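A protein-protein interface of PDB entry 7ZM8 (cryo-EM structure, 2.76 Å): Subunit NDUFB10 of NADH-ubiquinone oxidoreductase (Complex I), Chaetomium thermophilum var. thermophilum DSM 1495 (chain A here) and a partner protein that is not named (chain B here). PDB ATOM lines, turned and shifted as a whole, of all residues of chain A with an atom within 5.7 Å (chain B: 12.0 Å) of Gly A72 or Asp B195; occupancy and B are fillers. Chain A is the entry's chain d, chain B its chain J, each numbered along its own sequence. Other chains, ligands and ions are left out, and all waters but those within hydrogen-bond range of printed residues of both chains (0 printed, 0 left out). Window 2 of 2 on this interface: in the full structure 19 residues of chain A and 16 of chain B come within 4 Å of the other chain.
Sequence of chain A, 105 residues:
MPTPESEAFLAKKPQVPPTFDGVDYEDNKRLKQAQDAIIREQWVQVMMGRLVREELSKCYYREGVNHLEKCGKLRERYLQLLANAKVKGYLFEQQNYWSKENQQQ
Of chain B, only Ala B194 and Asp B195 come within 4 Å of Gly A72. No residue of chain B comes within 4 Å of Leu A74. Of chain B, only Ala B194 and Pro B196 come within 4 Å of Arg A75. Val B192 touches none of the printed residues of chain A. Of the printed residues of chain A, Cys B193 touches Glu A76. Of the printed residues of chain A, Ala B194 touches Gly A72 (3.8 Å) and Arg A75 (3.3 Å). Of chain A, only Gly A72 (3.5 Å), Lys A73 (3.8 Å) and Glu A76 (3.4 Å) come within 4 Å of Asp B195. Of the printed residues of chain A, Pro B196 touches Arg A75 (3.7 Å). Gln B198 touches none of the printed residues of chain A. The nearest residue of chain B that does not touch Gly A72 is Pro B196 (4.2 Å). The nearest residue of chain A that does not touch Asp B195 is Arg A75 (5.0 Å). The nearest printed residue of chain A that does not touch Ala B194 is Glu A76 (4.1 Å).
Printed residues of chain B that touch a printed residue of chain A: Cys B193, Ala B194, Asp B195 and Pro B196. Of the 10 printed residues of chain A, 4 touch a printed residue of chain B. Printed residues of chain A that touch a printed residue of chain B: Gly A72, Lys A73, Arg A75 and Glu A76.
Gly A72 touches Ala B194. Gly A72 touches Asp B195. Asp B195 touches Lys A73. Arg A75 touches Pro B196. CG of Glu A76 touches CB of Asp B195, 3.4 Å away.
The side-chain carboxylate of Asp B195 sits close to the backbone NH of Asp B197 (3.3 Å). The side-chain sulfur (SG) of Cys B193 lies within hydrogen-bond range of the backbone carbonyl oxygen (O) of Gln B198. The backbone carbonyl oxygen (O) of His A67 lies within hydrogen-bond range of the guanidinium group (NH2) of Arg A75 (3.1 Å). O of Asp B195 sits at hydrogen-bond distance from SG of Cys B193, at 3.2 Å.
NE of Arg A75 lies within hydrogen-bond range of O of Ala B194, 3.3 Å away. The side-chain carboxylate (OE2) of Glu A76 sits at hydrogen-bond distance from the side-chain sulfur (SG) of Cys B193, 3.2 Å away.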
ATOM      1  N   HIS A  67      15.653   6.573  -0.817  1.00  0.00           N
ATOM      2  CA  HIS A  67      14.648   5.786  -1.560  1.00  0.00           C
ATOM      3  C   HIS A  67      15.076   5.870  -3.023  1.00  0.00           C
ATOM      4  O   HIS A  67      14.683   5.004  -3.805  1.00  0.00           O
ATOM      5  CB  HIS A  67      13.268   6.433  -1.370  1.00  0.00           C
ATOM      6  CG  HIS A  67      13.109   7.753  -2.046  1.00  0.00           C
ATOM      7  ND1 HIS A  67      12.500   7.884  -3.278  1.00  0.00           N
ATOM      8  CD2 HIS A  67      13.480   8.995  -1.678  1.00  0.00           C
ATOM      9  CE1 HIS A  67      12.504   9.151  -3.635  1.00  0.00           C
ATOM     10  NE2 HIS A  67      13.101   9.850  -2.674  1.00  0.00           N
ATOM     11  N   GLU A  69      17.770   5.230  -4.300  1.00  0.00           N
ATOM     12  CA  GLU A  69      18.673   4.152  -4.655  1.00  0.00           C
ATOM     13  C   GLU A  69      18.246   2.809  -4.091  1.00  0.00           C
ATOM     14  O   GLU A  69      19.013   1.847  -4.189  1.00  0.00           O
ATOM     15  CB  GLU A  69      20.099   4.478  -4.195  1.00  0.00           C
ATOM     16  CG  GLU A  69      20.254   4.706  -2.714  1.00  0.00           C
ATOM     17  CD  GLU A  69      20.716   3.473  -1.968  1.00  0.00           C
ATOM     18  OE1 GLU A  69      21.257   2.552  -2.616  1.00  0.00           O
ATOM     19  OE2 GLU A  69      20.556   3.431  -0.730  1.00  0.00           O
ATOM     20  N   LYS A  70      17.052   2.711  -3.511  1.00  0.00           N
ATOM     21  CA  LYS A  70      16.559   1.465  -2.952  1.00  0.00           C
ATOM     22  C   LYS A  70      15.215   1.026  -3.502  1.00  0.00           C
ATOM     23  O   LYS A  70      14.842  -0.134  -3.303  1.00  0.00           O
ATOM     24  CB  LYS A  70      16.446   1.575  -1.424  1.00  0.00           C
ATOM     25  CG  LYS A  70      17.752   1.838  -0.716  1.00  0.00           C
ATOM     26  CD  LYS A  70      18.732   0.710  -0.940  1.00  0.00           C
ATOM     27  CE  LYS A  70      18.254  -0.565  -0.268  1.00  0.00           C
ATOM     28  NZ  LYS A  70      18.207  -0.420   1.214  1.00  0.00           N
ATOM     29  N   CYS A  71      14.480   1.907  -4.181  1.00  0.00           N
ATOM     30  CA  CYS A  71      13.123   1.616  -4.623  1.00  0.00           C
ATOM     31  C   CYS A  71      12.994   1.694  -6.142  1.00  0.00           C
ATOM     32  O   CYS A  71      11.912   1.956  -6.664  1.00  0.00           O
ATOM     33  CB  CYS A  71      12.124   2.558  -3.948  1.00  0.00           C
ATOM     34  SG  CYS A  71      12.208   2.658  -2.139  1.00  0.00           S
ATOM     35  N   GLY A  72      14.093   1.450  -6.862  1.00  0.00           N
ATOM     36  CA  GLY A  72      14.082   1.621  -8.306  1.00  0.00           C
ATOM     37  C   GLY A  72      13.360   0.532  -9.068  1.00  0.00           C
ATOM     38  O   GLY A  72      12.765   0.805 -10.115  1.00  0.00           O
ATOM     39  N   LYS A  73      13.409  -0.709  -8.574  1.00  0.00           N
ATOM     40  CA  LYS A  73      12.714  -1.802  -9.244  1.00  0.00           C
ATOM     41  C   LYS A  73      11.210  -1.596  -9.213  1.00  0.00           C
ATOM     42  O   LYS A  73      10.529  -1.808 -10.220  1.00  0.00           O
ATOM     43  CB  LYS A  73      13.085  -3.133  -8.593  1.00  0.00           C
ATOM     44  CG  LYS A  73      12.615  -4.352  -9.374  1.00  0.00           C
ATOM     45  CD  LYS A  73      13.296  -5.621  -8.893  1.00  0.00           C
ATOM     46  CE  LYS A  73      12.672  -6.127  -7.605  1.00  0.00           C
ATOM     47  NZ  LYS A  73      13.202  -7.465  -7.226  1.00  0.00           N
ATOM     48  N   LEU A  74      10.676  -1.183  -8.064  1.00  0.00           N
ATOM     49  CA  LEU A  74       9.255  -0.878  -7.966  1.00  0.00           C
ATOM     50  C   LEU A  74       8.890   0.318  -8.833  1.00  0.00           C
ATOM     51  O   LEU A  74       7.803   0.358  -9.419  1.00  0.00           O
ATOM     52  CB  LEU A  74       8.873  -0.621  -6.511  1.00  0.00           C
ATOM     53  CG  LEU A  74       8.615  -1.837  -5.623  1.00  0.00           C
ATOM     54  CD1 LEU A  74       8.480  -1.410  -4.180  1.00  0.00           C
ATOM     55  CD2 LEU A  74       7.370  -2.574  -6.073  1.00  0.00           C
ATOM     56  N   ARG A  75       9.778   1.307  -8.919  1.00  0.00           N
ATOM     57  CA  ARG A  75       9.525   2.455  -9.779  1.00  0.00           C
ATOM     58  C   ARG A  75       9.445   2.045 -11.243  1.00  0.00           C
ATOM     59  O   ARG A  75       8.598   2.547 -11.989  1.00  0.00           O
ATOM     60  CB  ARG A  75      10.612   3.505  -9.580  1.00  0.00           C
ATOM     61  CG  ARG A  75      10.392   4.408  -8.397  1.00  0.00           C
ATOM     62  CD  ARG A  75      11.328   5.569  -8.457  1.00  0.00           C
ATOM     63  NE  ARG A  75      12.708   5.145  -8.658  1.00  0.00           N
ATOM     64  CZ  ARG A  75      13.642   5.186  -7.719  1.00  0.00           C
ATOM     65  NH1 ARG A  75      14.871   4.788  -7.993  1.00  0.00           N
ATOM     66  NH2 ARG A  75      13.343   5.626  -6.508  1.00  0.00           N
ATOM     67  N   GLU A  76      10.330   1.145 -11.674  1.00  0.00           N
ATOM     68  CA  GLU A  76      10.260   0.611 -13.028  1.00  0.00           C
ATOM     69  C   GLU A  76       8.908  -0.019 -13.308  1.00  0.00           C
ATOM     70  O   GLU A  76       8.256   0.303 -14.305  1.00  0.00           O
ATOM     71  CB  GLU A  76      11.353  -0.433 -13.233  1.00  0.00           C
ATOM     72  CG  GLU A  76      12.709   0.093 -13.573  1.00  0.00           C
ATOM     73  CD  GLU A  76      12.807   0.554 -15.008  1.00  0.00           C
ATOM     74  OE1 GLU A  76      11.864   0.300 -15.789  1.00  0.00           O
ATOM     75  OE2 GLU A  76      13.859   1.113 -15.372  1.00  0.00           O
ATOM     76  N   ARG A  77       8.480  -0.935 -12.441  1.00  0.00           N
ATOM     77  CA  ARG A  77       7.258  -1.684 -12.700  1.00  0.00           C
ATOM     78  C   ARG A  77       6.048  -0.763 -12.753  1.00  0.00           C
ATOM     79  O   ARG A  77       5.171  -0.928 -13.605  1.00  0.00           O
ATOM     80  CB  ARG A  77       7.072  -2.758 -11.630  1.00  0.00           C
ATOM     81  CG  ARG A  77       6.003  -3.772 -11.953  1.00  0.00           C
ATOM     82  CD  ARG A  77       6.375  -4.573 -13.172  1.00  0.00           C
ATOM     83  NE  ARG A  77       5.237  -5.325 -13.685  1.00  0.00           N
ATOM     84  CZ  ARG A  77       4.717  -5.151 -14.893  1.00  0.00           C
ATOM     85  NH1 ARG A  77       3.678  -5.875 -15.277  1.00  0.00           N
ATOM     86  NH2 ARG A  77       5.237  -4.252 -15.713  1.00  0.00           N
ATOM     87  N   ASN B 190      14.018   9.254 -26.169  1.00  0.00           N
ATOM     88  CA  ASN B 190      14.766   8.233 -25.438  1.00  0.00           C
ATOM     89  C   ASN B 190      14.470   8.410 -23.960  1.00  0.00           C
ATOM     90  O   ASN B 190      15.215   9.081 -23.236  1.00  0.00           O
ATOM     91  CB  ASN B 190      16.266   8.331 -25.707  1.00  0.00           C
ATOM     92  CG  ASN B 190      17.044   7.164 -25.133  1.00  0.00           C
ATOM     93  OD1 ASN B 190      16.480   6.271 -24.501  1.00  0.00           O
ATOM     94  ND2 ASN B 190      18.354   7.169 -25.348  1.00  0.00           N
ATOM     95  N   PRO B 191      13.375   7.831 -23.475  1.00  0.00           N
ATOM     96  CA  PRO B 191      12.992   8.028 -22.073  1.00  0.00           C
ATOM     97  C   PRO B 191      14.010   7.441 -21.102  1.00  0.00           C
ATOM     98  O   PRO B 191      14.721   6.484 -21.412  1.00  0.00           O
ATOM     99  CB  PRO B 191      11.647   7.307 -21.983  1.00  0.00           C
ATOM    100  CG  PRO B 191      11.107   7.374 -23.357  1.00  0.00           C
ATOM    101  CD  PRO B 191      12.294   7.207 -24.250  1.00  0.00           C
ATOM    102  N   VAL B 192      14.077   8.042 -19.907  1.00  0.00           N
ATOM    103  CA  VAL B 192      15.087   7.653 -18.926  1.00  0.00           C
ATOM    104  C   VAL B 192      14.689   6.351 -18.237  1.00  0.00           C
ATOM    105  O   VAL B 192      13.546   5.887 -18.317  1.00  0.00           O
ATOM    106  CB  VAL B 192      15.331   8.774 -17.904  1.00  0.00           C
ATOM    107  CG1 VAL B 192      15.886   9.996 -18.588  1.00  0.00           C
ATOM    108  CG2 VAL B 192      14.044   9.121 -17.189  1.00  0.00           C
ATOM    109  N   CYS B 193      15.661   5.750 -17.548  1.00  0.00           N
ATOM    110  CA  CYS B 193      15.495   4.387 -17.056  1.00  0.00           C
ATOM    111  C   CYS B 193      14.523   4.326 -15.886  1.00  0.00           C
ATOM    112  O   CYS B 193      13.522   3.604 -15.941  1.00  0.00           O
ATOM    113  CB  CYS B 193      16.852   3.814 -16.658  1.00  0.00           C
ATOM    114  SG  CYS B 193      16.778   2.168 -15.933  1.00  0.00           S
ATOM    115  N   ALA B 194      14.786   5.108 -14.839  1.00  0.00           N
ATOM    116  CA  ALA B 194      14.118   5.139 -13.525  1.00  0.00           C
ATOM    117  C   ALA B 194      14.618   4.069 -12.567  1.00  0.00           C
ATOM    118  O   ALA B 194      14.153   4.033 -11.426  1.00  0.00           O
ATOM    119  CB  ALA B 194      12.592   5.032 -13.598  1.00  0.00           C
ATOM    120  N   ASP B 195      15.562   3.219 -12.966  1.00  0.00           N
ATOM    121  CA  ASP B 195      16.183   2.267 -12.050  1.00  0.00           C
ATOM    122  C   ASP B 195      17.692   2.464 -12.075  1.00  0.00           C
ATOM    123  O   ASP B 195      18.312   2.344 -13.152  1.00  0.00           O
ATOM    124  CB  ASP B 195      15.828   0.829 -12.410  1.00  0.00           C
ATOM    125  CG  ASP B 195      16.154  -0.145 -11.300  1.00  0.00           C
ATOM    126  OD1 ASP B 195      16.629   0.301 -10.237  1.00  0.00           O
ATOM    127  OD2 ASP B 195      15.926  -1.357 -11.487  1.00  0.00           O
ATOM    128  N   PRO B 196      18.323   2.764 -10.940  1.00  0.00           N
ATOM    129  CA  PRO B 196      19.790   2.841 -10.922  1.00  0.00           C
ATOM    130  C   PRO B 196      20.468   1.551 -11.336  1.00  0.00           C
ATOM    131  O   PRO B 196      21.599   1.589 -11.838  1.00  0.00           O
ATOM    132  CB  PRO B 196      20.097   3.200  -9.466  1.00  0.00           C
ATOM    133  CG  PRO B 196      18.890   3.920  -9.008  1.00  0.00           C
ATOM    134  CD  PRO B 196      17.727   3.281  -9.700  1.00  0.00           C
ATOM    135  N   ASP B 197      19.823   0.407 -11.138  1.00  0.00           N
ATOM    136  CA  ASP B 197      20.364  -0.881 -11.549  1.00  0.00           C
ATOM    137  C   ASP B 197      19.689  -1.314 -12.843  1.00  0.00           C
ATOM    138  O   ASP B 197      18.456  -1.366 -12.916  1.00  0.00           O
ATOM    139  CB  ASP B 197      20.164  -1.930 -10.456  1.00  0.00           C
ATOM    140  CG  ASP B 197      21.014  -1.663  -9.232  1.00  0.00           C
ATOM    141  OD1 ASP B 197      22.102  -1.072  -9.383  1.00  0.00           O
ATOM    142  OD2 ASP B 197      20.594  -2.042  -8.118  1.00  0.00           O
ATOM    143  N   GLN B 198      20.498  -1.618 -13.856  1.00  0.00           N
ATOM    144  CA  GLN B 198      20.008  -2.048 -15.164  1.00  0.00           C
ATOM    145  C   GLN B 198      19.034  -1.039 -15.766  1.00  0.00           C
ATOM    146  O   GLN B 198      17.973  -1.411 -16.267  1.00  0.00           O
ATOM    147  CB  GLN B 198      19.341  -3.424 -15.063  1.00  0.00           C
